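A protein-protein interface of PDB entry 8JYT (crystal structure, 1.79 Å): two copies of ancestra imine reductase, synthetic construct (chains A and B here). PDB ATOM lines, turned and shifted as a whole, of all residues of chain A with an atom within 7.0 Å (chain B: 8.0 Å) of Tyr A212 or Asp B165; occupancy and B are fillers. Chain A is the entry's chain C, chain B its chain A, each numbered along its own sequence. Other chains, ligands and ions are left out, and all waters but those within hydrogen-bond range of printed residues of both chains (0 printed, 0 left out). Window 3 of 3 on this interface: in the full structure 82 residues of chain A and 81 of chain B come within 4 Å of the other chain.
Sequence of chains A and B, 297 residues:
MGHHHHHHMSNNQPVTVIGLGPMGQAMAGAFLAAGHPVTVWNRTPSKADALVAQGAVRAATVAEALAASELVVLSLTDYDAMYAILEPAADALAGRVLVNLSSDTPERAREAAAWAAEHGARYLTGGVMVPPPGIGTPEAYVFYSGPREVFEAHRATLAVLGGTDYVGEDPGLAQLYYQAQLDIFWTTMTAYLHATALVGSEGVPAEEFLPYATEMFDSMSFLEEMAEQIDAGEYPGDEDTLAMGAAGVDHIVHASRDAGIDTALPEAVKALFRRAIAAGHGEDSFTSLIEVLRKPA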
ATOM      1  N   VAL A 204      11.952  -9.911   6.717  1.00  0.00           N
ATOM      2  CA  VAL A 204      12.027 -10.549   5.412  1.00  0.00           C
ATOM      3  C   VAL A 204      11.390 -11.930   5.519  1.00  0.00           C
ATOM      4  O   VAL A 204      11.906 -12.781   6.258  1.00  0.00           O
ATOM      5  CB  VAL A 204      13.480 -10.644   4.927  1.00  0.00           C
ATOM      6  CG1 VAL A 204      13.533 -11.333   3.586  1.00  0.00           C
ATOM      7  CG2 VAL A 204      14.106  -9.269   4.871  1.00  0.00           C
ATOM      8  N   GLU A 208      10.654 -15.112   0.795  1.00  0.00           N
ATOM      9  CA  GLU A 208      11.296 -14.037   0.052  1.00  0.00           C
ATOM     10  C   GLU A 208      12.803 -14.230  -0.046  1.00  0.00           C
ATOM     11  O   GLU A 208      13.404 -13.855  -1.063  1.00  0.00           O
ATOM     12  CB  GLU A 208      10.993 -12.697   0.727  1.00  0.00           C
ATOM     13  CG  GLU A 208      11.240 -11.480  -0.128  1.00  0.00           C
ATOM     14  CD  GLU A 208      10.628 -10.231   0.472  1.00  0.00           C
ATOM     15  OE1 GLU A 208       9.385 -10.110   0.462  1.00  0.00           O
ATOM     16  OE2 GLU A 208      11.394  -9.369   0.944  1.00  0.00           O
ATOM     17  N   PHE A 209      13.423 -14.790   0.999  1.00  0.00           N
ATOM     18  CA  PHE A 209      14.845 -15.109   0.973  1.00  0.00           C
ATOM     19  C   PHE A 209      15.123 -16.423   0.251  1.00  0.00           C
ATOM     20  O   PHE A 209      16.233 -16.627  -0.265  1.00  0.00           O
ATOM     21  CB  PHE A 209      15.389 -15.158   2.414  1.00  0.00           C
ATOM     22  CG  PHE A 209      16.872 -15.362   2.498  1.00  0.00           C
ATOM     23  CD1 PHE A 209      17.746 -14.407   2.000  1.00  0.00           C
ATOM     24  CD2 PHE A 209      17.397 -16.512   3.072  1.00  0.00           C
ATOM     25  CE1 PHE A 209      19.110 -14.587   2.067  1.00  0.00           C
ATOM     26  CE2 PHE A 209      18.776 -16.703   3.134  1.00  0.00           C
ATOM     27  CZ  PHE A 209      19.631 -15.723   2.620  1.00  0.00           C
ATOM     28  N   LEU A 210      14.140 -17.322   0.204  1.00  0.00           N
ATOM     29  CA  LEU A 210      14.333 -18.631  -0.417  1.00  0.00           C
ATOM     30  C   LEU A 210      15.037 -18.580  -1.766  1.00  0.00           C
ATOM     31  O   LEU A 210      15.962 -19.377  -1.977  1.00  0.00           O
ATOM     32  CB  LEU A 210      12.978 -19.327  -0.615  1.00  0.00           C
ATOM     33  CG  LEU A 210      12.987 -20.787  -1.078  1.00  0.00           C
ATOM     34  CD1 LEU A 210      13.825 -21.684  -0.170  1.00  0.00           C
ATOM     35  CD2 LEU A 210      11.558 -21.326  -1.186  1.00  0.00           C
ATOM     36  N   PRO A 211      14.649 -17.717  -2.714  1.00  0.00           N
ATOM     37  CA  PRO A 211      15.361 -17.693  -4.010  1.00  0.00           C
ATOM     38  C   PRO A 211      16.859 -17.487  -3.854  1.00  0.00           C
ATOM     39  O   PRO A 211      17.666 -18.102  -4.562  1.00  0.00           O
ATOM     40  CB  PRO A 211      14.708 -16.509  -4.745  1.00  0.00           C
ATOM     41  CG  PRO A 211      13.340 -16.382  -4.113  1.00  0.00           C
ATOM     42  CD  PRO A 211      13.580 -16.701  -2.650  1.00  0.00           C
ATOM     43  N   TYR A 212      17.249 -16.586  -2.955  1.00  0.00           N
ATOM     44  CA  TYR A 212      18.660 -16.298  -2.755  1.00  0.00           C
ATOM     45  C   TYR A 212      19.376 -17.473  -2.099  1.00  0.00           C
ATOM     46  O   TYR A 212      20.514 -17.792  -2.455  1.00  0.00           O
ATOM     47  CB  TYR A 212      18.784 -15.045  -1.905  1.00  0.00           C
ATOM     48  CG  TYR A 212      18.125 -13.846  -2.529  1.00  0.00           C
ATOM     49  CD1 TYR A 212      18.686 -13.206  -3.618  1.00  0.00           C
ATOM     50  CD2 TYR A 212      16.927 -13.366  -2.035  1.00  0.00           C
ATOM     51  CE1 TYR A 212      18.088 -12.117  -4.178  1.00  0.00           C
ATOM     52  CE2 TYR A 212      16.324 -12.273  -2.593  1.00  0.00           C
ATOM     53  CZ  TYR A 212      16.907 -11.663  -3.675  1.00  0.00           C
ATOM     54  OH  TYR A 212      16.308 -10.564  -4.233  1.00  0.00           O
ATOM     55  N   ALA A 213      18.741 -18.115  -1.117  1.00  0.00           N
ATOM     56  CA  ALA A 213      19.343 -19.308  -0.531  1.00  0.00           C
ATOM     57  C   ALA A 213      19.486 -20.405  -1.580  1.00  0.00           C
ATOM     58  O   ALA A 213      20.524 -21.075  -1.662  1.00  0.00           O
ATOM     59  CB  ALA A 213      18.501 -19.780   0.654  1.00  0.00           C
ATOM     60  N   THR A 214      18.452 -20.598  -2.399  1.00  0.00           N
ATOM     61  CA  THR A 214      18.496 -21.651  -3.409  1.00  0.00           C
ATOM     62  C   THR A 214      19.622 -21.414  -4.405  1.00  0.00           C
ATOM     63  O   THR A 214      20.332 -22.354  -4.789  1.00  0.00           O
ATOM     64  CB  THR A 214      17.153 -21.741  -4.135  1.00  0.00           C
ATOM     65  OG1 THR A 214      16.162 -22.299  -3.260  1.00  0.00           O
ATOM     66  CG2 THR A 214      17.272 -22.588  -5.389  1.00  0.00           C
ATOM     67  N   GLU A 215      19.799 -20.172  -4.845  1.00  0.00           N
ATOM     68  CA  GLU A 215      20.865 -19.900  -5.798  1.00  0.00           C
ATOM     69  C   GLU A 215      22.244 -19.972  -5.153  1.00  0.00           C
ATOM     70  O   GLU A 215      23.229 -20.238  -5.850  1.00  0.00           O
ATOM     71  CB  GLU A 215      20.674 -18.531  -6.449  1.00  0.00           C
ATOM     72  CG  GLU A 215      20.770 -17.359  -5.516  1.00  0.00           C
ATOM     73  CD  GLU A 215      20.536 -16.044  -6.241  1.00  0.00           C
ATOM     74  OE1 GLU A 215      20.827 -15.964  -7.454  1.00  0.00           O
ATOM     75  OE2 GLU A 215      20.072 -15.085  -5.602  1.00  0.00           O
ATOM     76  N   MET A 216      22.339 -19.739  -3.841  1.00  0.00           N
ATOM     77  CA  MET A 216      23.607 -19.955  -3.151  1.00  0.00           C
ATOM     78  C   MET A 216      24.079 -21.397  -3.336  1.00  0.00           C
ATOM     79  O   MET A 216      25.244 -21.642  -3.670  1.00  0.00           O
ATOM     80  CB  MET A 216      23.476 -19.609  -1.657  1.00  0.00           C
ATOM     81  CG  MET A 216      24.679 -20.125  -0.870  1.00  0.00           C
ATOM     82  SD  MET A 216      26.215 -19.210  -1.256  1.00  0.00           S
ATOM     83  CE  MET A 216      25.568 -17.589  -1.652  1.00  0.00           C
ATOM     84  N   PHE A 217      23.182 -22.363  -3.115  1.00  0.00           N
ATOM     85  CA  PHE A 217      23.546 -23.771  -3.220  1.00  0.00           C
ATOM     86  C   PHE A 217      23.860 -24.160  -4.660  1.00  0.00           C
ATOM     87  O   PHE A 217      24.749 -24.986  -4.896  1.00  0.00           O
ATOM     88  CB  PHE A 217      22.410 -24.623  -2.662  1.00  0.00           C
ATOM     89  CG  PHE A 217      22.294 -24.559  -1.163  1.00  0.00           C
ATOM     90  CD1 PHE A 217      23.358 -24.909  -0.353  1.00  0.00           C
ATOM     91  CD2 PHE A 217      21.114 -24.150  -0.565  1.00  0.00           C
ATOM     92  CE1 PHE A 217      23.252 -24.851   1.021  1.00  0.00           C
ATOM     93  CE2 PHE A 217      20.998 -24.089   0.815  1.00  0.00           C
ATOM     94  CZ  PHE A 217      22.069 -24.443   1.609  1.00  0.00           C
ATOM     95  N   THR B 125      24.058   1.007   0.394  1.00  0.00           N
ATOM     96  CA  THR B 125      24.820  -0.136   0.844  1.00  0.00           C
ATOM     97  C   THR B 125      24.769  -1.194  -0.241  1.00  0.00           C
ATOM     98  O   THR B 125      23.741  -1.387  -0.897  1.00  0.00           O
ATOM     99  CB  THR B 125      24.252  -0.687   2.160  1.00  0.00           C
ATOM    100  OG1 THR B 125      24.143   0.374   3.126  1.00  0.00           O
ATOM    101  CG2 THR B 125      25.152  -1.807   2.711  1.00  0.00           C
ATOM    102  N   GLY B 126      25.878  -1.872  -0.439  1.00  0.00           N
ATOM    103  CA  GLY B 126      25.914  -2.945  -1.395  1.00  0.00           C
ATOM    104  C   GLY B 126      26.600  -4.175  -0.830  1.00  0.00           C
ATOM    105  O   GLY B 126      27.558  -4.077  -0.065  1.00  0.00           O
ATOM    106  N   GLY B 127      26.130  -5.325  -1.295  1.00  0.00           N
ATOM    107  CA  GLY B 127      26.776  -6.595  -1.004  1.00  0.00           C
ATOM    108  C   GLY B 127      27.043  -7.424  -2.239  1.00  0.00           C
ATOM    109  O   GLY B 127      26.117  -7.889  -2.914  1.00  0.00           O
ATOM    110  N   MET B 129      28.181 -10.445  -4.451  1.00  0.00           N
ATOM    111  CA  MET B 129      28.096 -11.891  -4.312  1.00  0.00           C
ATOM    112  C   MET B 129      28.936 -12.640  -5.339  1.00  0.00           C
ATOM    113  O   MET B 129      28.570 -13.759  -5.716  1.00  0.00           O
ATOM    114  CB  MET B 129      26.635 -12.325  -4.414  1.00  0.00           C
ATOM    115  CG  MET B 129      25.753 -12.001  -3.207  1.00  0.00           C
ATOM    116  SD  MET B 129      26.521 -12.476  -1.653  1.00  0.00           S
ATOM    117  CE  MET B 129      26.641 -14.236  -1.825  1.00  0.00           C
ATOM    118  N   ALA B 140      26.712 -12.107 -12.461  1.00  0.00           N
ATOM    119  CA  ALA B 140      26.985 -11.616 -11.117  1.00  0.00           C
ATOM    120  C   ALA B 140      25.800 -10.787 -10.624  1.00  0.00           C
ATOM    121  O   ALA B 140      24.952 -10.349 -11.406  1.00  0.00           O
ATOM    122  CB  ALA B 140      28.262 -10.759 -11.105  1.00  0.00           C
ATOM    123  N   TYR B 141      25.740 -10.578  -9.307  1.00  0.00           N
ATOM    124  CA  TYR B 141      24.706  -9.730  -8.732  1.00  0.00           C
ATOM    125  C   TYR B 141      25.200  -9.101  -7.439  1.00  0.00           C
ATOM    126  O   TYR B 141      26.122  -9.606  -6.786  1.00  0.00           O
ATOM    127  CB  TYR B 141      23.394 -10.499  -8.498  1.00  0.00           C
ATOM    128  CG  TYR B 141      23.438 -11.495  -7.357  1.00  0.00           C
ATOM    129  CD1 TYR B 141      24.092 -12.719  -7.499  1.00  0.00           C
ATOM    130  CD2 TYR B 141      22.805 -11.234  -6.145  1.00  0.00           C
ATOM    131  CE1 TYR B 141      24.134 -13.639  -6.460  1.00  0.00           C
ATOM    132  CE2 TYR B 141      22.832 -12.167  -5.101  1.00  0.00           C
ATOM    133  CZ  TYR B 141      23.501 -13.355  -5.274  1.00  0.00           C
ATOM    134  OH  TYR B 141      23.551 -14.279  -4.265  1.00  0.00           O
ATOM    135  N   VAL B 142      24.584  -7.967  -7.103  1.00  0.00           N
ATOM    136  CA  VAL B 142      24.956  -7.156  -5.951  1.00  0.00           C
ATOM    137  C   VAL B 142      23.666  -6.739  -5.249  1.00  0.00           C
ATOM    138  O   VAL B 142      22.761  -6.175  -5.883  1.00  0.00           O
ATOM    139  CB  VAL B 142      25.781  -5.910  -6.351  1.00  0.00           C
ATOM    140  CG1 VAL B 142      26.101  -5.046  -5.133  1.00  0.00           C
ATOM    141  CG2 VAL B 142      27.053  -6.305  -7.082  1.00  0.00           C
ATOM    142  N   PHE B 143      23.576  -7.031  -3.950  1.00  0.00           N
ATOM    143  CA  PHE B 143      22.479  -6.516  -3.138  1.00  0.00           C
ATOM    144  C   PHE B 143      22.661  -5.011  -2.953  1.00  0.00           C
ATOM    145  O   PHE B 143      23.759  -4.552  -2.639  1.00  0.00           O
ATOM    146  CB  PHE B 143      22.458  -7.177  -1.760  1.00  0.00           C
ATOM    147  CG  PHE B 143      22.069  -8.626  -1.796  1.00  0.00           C
ATOM    148  CD1 PHE B 143      20.794  -9.011  -2.155  1.00  0.00           C
ATOM    149  CD2 PHE B 143      22.988  -9.613  -1.455  1.00  0.00           C
ATOM    150  CE1 PHE B 143      20.436 -10.348  -2.173  1.00  0.00           C
ATOM    151  CE2 PHE B 143      22.628 -10.956  -1.477  1.00  0.00           C
ATOM    152  CZ  PHE B 143      21.350 -11.315  -1.841  1.00  0.00           C
ATOM    153  N   TYR B 144      21.564  -4.248  -3.056  1.00  0.00           N
ATOM    154  CA  TYR B 144      21.572  -2.813  -2.781  1.00  0.00           C
ATOM    155  C   TYR B 144      20.449  -2.434  -1.823  1.00  0.00           C
ATOM    156  O   TYR B 144      19.328  -2.938  -1.936  1.00  0.00           O
ATOM    157  CB  TYR B 144      21.417  -2.034  -4.080  1.00  0.00           C
ATOM    158  CG  TYR B 144      22.643  -2.104  -4.952  1.00  0.00           C
ATOM    159  CD1 TYR B 144      23.822  -1.449  -4.599  1.00  0.00           C
ATOM    160  CD2 TYR B 144      22.638  -2.878  -6.122  1.00  0.00           C
ATOM    161  CE1 TYR B 144      24.963  -1.547  -5.414  1.00  0.00           C
ATOM    162  CE2 TYR B 144      23.767  -2.979  -6.930  1.00  0.00           C
ATOM    163  CZ  TYR B 144      24.915  -2.314  -6.566  1.00  0.00           C
ATOM    164  OH  TYR B 144      26.023  -2.446  -7.367  1.00  0.00           O
ATOM    165  N   SER B 145      20.752  -1.530  -0.889  1.00  0.00           N
ATOM    166  CA  SER B 145      19.731  -0.968  -0.012  1.00  0.00           C
ATOM    167  C   SER B 145      20.059   0.488   0.292  1.00  0.00           C
ATOM    168  O   SER B 145      21.224   0.899   0.272  1.00  0.00           O
ATOM    169  CB  SER B 145      19.583  -1.782   1.296  1.00  0.00           C
ATOM    170  OG  SER B 145      20.705  -1.638   2.169  1.00  0.00           O
ATOM    171  N   PHE B 151      19.172   4.841  -5.579  1.00  0.00           N
ATOM    172  CA  PHE B 151      19.476   3.629  -6.329  1.00  0.00           C
ATOM    173  C   PHE B 151      18.955   3.733  -7.761  1.00  0.00           C
ATOM    174  O   PHE B 151      19.655   3.359  -8.709  1.00  0.00           O
ATOM    175  CB  PHE B 151      18.900   2.399  -5.621  1.00  0.00           C
ATOM    176  CG  PHE B 151      18.856   1.180  -6.491  1.00  0.00           C
ATOM    177  CD1 PHE B 151      19.969   0.379  -6.616  1.00  0.00           C
ATOM    178  CD2 PHE B 151      17.710   0.835  -7.175  1.00  0.00           C
ATOM    179  CE1 PHE B 151      19.943  -0.737  -7.405  1.00  0.00           C
ATOM    180  CE2 PHE B 151      17.687  -0.271  -7.995  1.00  0.00           C
ATOM    181  CZ  PHE B 151      18.799  -1.067  -8.099  1.00  0.00           C
ATOM    182  N   LEU B 158      25.818   1.123 -11.908  1.00  0.00           N
ATOM    183  CA  LEU B 158      26.010  -0.008 -11.017  1.00  0.00           C
ATOM    184  C   LEU B 158      25.824  -1.326 -11.754  1.00  0.00           C
ATOM    185  O   LEU B 158      26.488  -2.320 -11.430  1.00  0.00           O
ATOM    186  CB  LEU B 158      25.026   0.102  -9.854  1.00  0.00           C
ATOM    187  CG  LEU B 158      25.238   1.307  -8.930  1.00  0.00           C
ATOM    188  CD1 LEU B 158      24.124   1.394  -7.880  1.00  0.00           C
ATOM    189  CD2 LEU B 158      26.606   1.243  -8.268  1.00  0.00           C
ATOM    190  N   GLY B 162      27.231  -5.998 -12.516  1.00  0.00           N
ATOM    191  CA  GLY B 162      26.405  -7.182 -12.432  1.00  0.00           C
ATOM    192  C   GLY B 162      24.988  -6.777 -12.092  1.00  0.00           C
ATOM    193  O   GLY B 162      24.650  -5.597 -12.043  1.00  0.00           O
ATOM    194  N   GLY B 163      24.161  -7.787 -11.864  1.00  0.00           N
ATOM    195  CA  GLY B 163      22.783  -7.547 -11.494  1.00  0.00           C
ATOM    196  C   GLY B 163      22.650  -6.585 -10.334  1.00  0.00           C
ATOM    197  O   GLY B 163      23.481  -6.602  -9.417  1.00  0.00           O
ATOM    198  N   THR B 164      21.617  -5.735 -10.381  1.00  0.00           N
ATOM    199  CA  THR B 164      21.325  -4.758  -9.334  1.00  0.00           C
ATOM    200  C   THR B 164      20.117  -5.271  -8.559  1.00  0.00           C
ATOM    201  O   THR B 164      18.990  -5.251  -9.071  1.00  0.00           O
ATOM    202  CB  THR B 164      21.024  -3.383  -9.921  1.00  0.00           C
ATOM    203  OG1 THR B 164      20.034  -3.521 -10.945  1.00  0.00           O
ATOM    204  CG2 THR B 164      22.283  -2.767 -10.505  1.00  0.00           C
ATOM    205  N   ASP B 165      20.339  -5.724  -7.329  1.00  0.00           N
ATOM    206  CA  ASP B 165      19.304  -6.406  -6.560  1.00  0.00           C
ATOM    207  C   ASP B 165      18.929  -5.549  -5.344  1.00  0.00           C
ATOM    208  O   ASP B 165      19.499  -5.695  -4.261  1.00  0.00           O
ATOM    209  CB  ASP B 165      19.817  -7.787  -6.146  1.00  0.00           C
ATOM    210  CG  ASP B 165      18.744  -8.830  -6.173  1.00  0.00           C
ATOM    211  OD1 ASP B 165      17.954  -8.883  -5.219  1.00  0.00           O
ATOM    212  OD2 ASP B 165      18.705  -9.612  -7.157  1.00  0.00           O
ATOM    213  N   TYR B 166      17.959  -4.662  -5.537  1.00  0.00           N
ATOM    214  CA  TYR B 166      17.537  -3.716  -4.515  1.00  0.00           C
ATOM    215  C   TYR B 166      16.636  -4.411  -3.515  1.00  0.00           C
ATOM    216  O   TYR B 166      15.621  -4.993  -3.899  1.00  0.00           O
ATOM    217  CB  TYR B 166      16.807  -2.538  -5.159  1.00  0.00           C
ATOM    218  CG  TYR B 166      16.367  -1.459  -4.182  1.00  0.00           C
ATOM    219  CD1 TYR B 166      17.273  -0.575  -3.610  1.00  0.00           C
ATOM    220  CD2 TYR B 166      15.017  -1.338  -3.819  1.00  0.00           C
ATOM    221  CE1 TYR B 166      16.844   0.402  -2.723  1.00  0.00           C
ATOM    222  CE2 TYR B 166      14.595  -0.366  -2.934  1.00  0.00           C
ATOM    223  CZ  TYR B 166      15.511   0.485  -2.387  1.00  0.00           C
ATOM    224  OH  TYR B 166      15.085   1.448  -1.511  1.00  0.00           O
ATOM    225  N   VAL B 167      16.993  -4.323  -2.236  1.00  0.00           N
ATOM    226  CA  VAL B 167      16.287  -5.057  -1.187  1.00  0.00           C
ATOM    227  C   VAL B 167      15.523  -4.153  -0.223  1.00  0.00           C
ATOM    228  O   VAL B 167      14.796  -4.673   0.644  1.00  0.00           O
ATOM    229  CB  VAL B 167      17.251  -5.973  -0.399  1.00  0.00           C
ATOM    230  CG1 VAL B 167      17.673  -7.187  -1.249  1.00  0.00           C
ATOM    231  CG2 VAL B 167      18.467  -5.214   0.105  1.00  0.00           C
ATOM    232  N   GLY B 168      15.651  -2.843  -0.331  1.00  0.00           N
ATOM    233  CA  GLY B 168      14.836  -1.968   0.490  1.00  0.00           C
ATOM    234  C   GLY B 168      15.568  -0.711   0.918  1.00  0.00           C
ATOM    235  O   GLY B 168      16.718  -0.464   0.567  1.00  0.00           O
ATOM    236  N   LEU B 173      19.969  -3.491   5.106  1.00  0.00           N
ATOM    237  CA  LEU B 173      19.384  -4.669   4.477  1.00  0.00           C
ATOM    238  C   LEU B 173      20.348  -5.343   3.502  1.00  0.00           C
ATOM    239  O   LEU B 173      20.438  -6.567   3.466  1.00  0.00           O
ATOM    240  CB  LEU B 173      18.107  -4.275   3.755  1.00  0.00           C
ATOM    241  CG  LEU B 173      16.823  -4.175   4.554  1.00  0.00           C
ATOM    242  CD1 LEU B 173      15.711  -3.521   3.770  1.00  0.00           C
ATOM    243  CD2 LEU B 173      16.394  -5.569   5.056  1.00  0.00           C
ATOM    244  N   ALA B 174      21.063  -4.572   2.673  1.00  0.00           N
ATOM    245  CA  ALA B 174      21.939  -5.217   1.688  1.00  0.00           C
ATOM    246  C   ALA B 174      22.979  -6.094   2.377  1.00  0.00           C
ATOM    247  O   ALA B 174      23.278  -7.207   1.920  1.00  0.00           O
ATOM    248  CB  ALA B 174      22.603  -4.160   0.800  1.00  0.00           C
ATOM    249  N   TYR B 177      21.210  -9.346   3.856  1.00  0.00           N
ATOM    250  CA  TYR B 177      21.091 -10.390   2.840  1.00  0.00           C
ATOM    251  C   TYR B 177      22.449 -11.024   2.552  1.00  0.00           C
ATOM    252  O   TYR B 177      22.558 -12.249   2.439  1.00  0.00           O
ATOM    253  CB  TYR B 177      20.482  -9.801   1.560  1.00  0.00           C
ATOM    254  CG  TYR B 177      18.968  -9.735   1.499  1.00  0.00           C
ATOM    255  CD1 TYR B 177      18.275  -8.729   2.149  1.00  0.00           C
ATOM    256  CD2 TYR B 177      18.245 -10.631   0.726  1.00  0.00           C
ATOM    257  CE1 TYR B 177      16.878  -8.653   2.095  1.00  0.00           C
ATOM    258  CE2 TYR B 177      16.860 -10.546   0.643  1.00  0.00           C
ATOM    259  CZ  TYR B 177      16.190  -9.549   1.330  1.00  0.00           C
ATOM    260  OH  TYR B 177      14.829  -9.457   1.250  1.00  0.00           O
ATOM    261  N   ALA B 180      23.745 -13.221   5.437  1.00  0.00           N
ATOM    262  CA  ALA B 180      22.957 -14.448   5.476  1.00  0.00           C
ATOM    263  C   ALA B 180      23.382 -15.421   4.388  1.00  0.00           C
ATOM    264  O   ALA B 180      23.428 -16.628   4.615  1.00  0.00           O
ATOM    265  CB  ALA B 180      21.471 -14.125   5.349  1.00  0.00           C
ATOM    266  N   GLN B 181      23.656 -14.923   3.183  1.00  0.00           N
ATOM    267  CA  GLN B 181      24.140 -15.792   2.129  1.00  0.00           C
ATOM    268  C   GLN B 181      25.495 -16.375   2.501  1.00  0.00           C
ATOM    269  O   GLN B 181      25.739 -17.564   2.293  1.00  0.00           O
ATOM    270  CB  GLN B 181      24.254 -15.002   0.829  1.00  0.00           C
ATOM    271  CG  GLN B 181      22.921 -14.687   0.185  1.00  0.00           C
ATOM    272  CD  GLN B 181      22.442 -15.781  -0.690  1.00  0.00           C
ATOM    273  OE1 GLN B 181      21.885 -16.758  -0.181  1.00  0.00           O
ATOM    274  NE2 GLN B 181      22.615 -15.640  -2.006  1.00  0.00           N
ATOM    275  N   ILE B 184      25.135 -19.193   5.022  1.00  0.00           N
ATOM    276  CA  ILE B 184      24.903 -20.466   4.365  1.00  0.00           C
ATOM    277  C   ILE B 184      26.190 -20.992   3.752  1.00  0.00           C
ATOM    278  O   ILE B 184      26.513 -22.175   3.878  1.00  0.00           O
ATOM    279  CB  ILE B 184      23.796 -20.330   3.311  1.00  0.00           C
ATOM    280  CG1 ILE B 184      22.445 -20.082   3.984  1.00  0.00           C
ATOM    281  CG2 ILE B 184      23.736 -21.573   2.454  1.00  0.00           C
ATOM    282  CD1 ILE B 184      21.376 -19.640   3.035  1.00  0.00           C
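Printed residues of chain B within 4 Å of Phe A209: Ala B180, Gln B181 and Ile B184.
Of chain B, only Phe B143, Asp B165, Tyr B177 and Gln B181 come within 4 Å of Tyr A212.
Of chain B, only Gln B181 and Ile B184 come within 4 Å of Ala A213.
Of the printed residues of chain B, Glu A215 touches Tyr B141 (3.8 Å).
Of the printed residues of chain B, Met A216 touches Met B129, Gln B181 and Ile B184.
Thr B125 touches none of the printed residues of chain A.
Of the printed residues of chain A, Met B129 touches Met A216.
Of chain A, only Tyr A212 (2.6 Å) comes within 4 Å of Asp B165.
Tyr B166 touches none of the printed residues of chain A.
The nearest residue of chain B that does not touch Tyr A212 is Tyr B141 (4.5 Å).
The nearest residue of chain A that does not touch Asp B165 is Glu A215 (5.9 Å).
Among the printed residues, merely in contact across the chains: Val A204 with Tyr B177 (3.3 Å), Phe A217 with Ile B184 (3.4 Å), Met A216 with Met B129 (3.5 Å), Ala A213 with Gln B181 (3.5 Å), Met A216 with Gln B181 (3.6 Å), Tyr A212 with Phe B143 (3.6 Å), Phe A209 with Ala B180 (3.7 Å), Tyr A212 with Tyr B177 (3.7 Å), Ala A213 with Ile B184 (3.7 Å), Phe A209 with Gln B181 (3.7 Å), Met A216 with Ile B184 (3.7 Å), Glu A215 with Tyr B141 (3.8 Å) and Phe A209 with Ile B184 (3.9 Å).
No position is printed for both chains.
Of the 16 pairs that touch across the chains among the printed residues, none has its exchanged pair printed and touching as well.
Hydrophobic or aromatic side chains of chain A within 4 Å of the printed part of chain B: Val A204, Phe A209, Tyr A212, Ala A213, Met A216 and Phe A217.
Hydrophobic or aromatic side chains of chain B within 4 Å of the printed part of chain A: Met B129, Tyr B141, Phe B143, Tyr B177, Ala B180 and Ile B184.
Among the printed residues, no Asp or Glu carboxylate lies within 4 Å of a Lys or Arg side-chain nitrogen of the other chain.
OD1 of Asp B165 lies within hydrogen-bond range of OH of Tyr A212.
The side-chain hydroxyl of Tyr B177 lies within hydrogen-bond range of the side-chain carboxylate of Glu A208 (3.4 Å).
The backbone carbonyl oxygen (O) of Tyr A212 sits close to the side-chain amide oxygen (OE1) of Gln B181 (2.8 Å).
N of Gly B127 is in hydrogen-bond range of O of Phe B143, 2.8 Å away.
N of Met B129 is in hydrogen-bond range of O of Tyr B141, 3.2 Å away.
The side-chain hydroxyl (OH) of Tyr B141 lies within hydrogen-bond range of the side-chain amide nitrogen (NE2) of Gln B181.
The backbone carbonyl oxygen (O) of Val B142 lies within hydrogen-bond range of the backbone NH (N) of Asp B165, 2.9 Å away.
The backbone carbonyl oxygen of Asp B165 lies within hydrogen-bond range of the backbone NH of Tyr B144.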
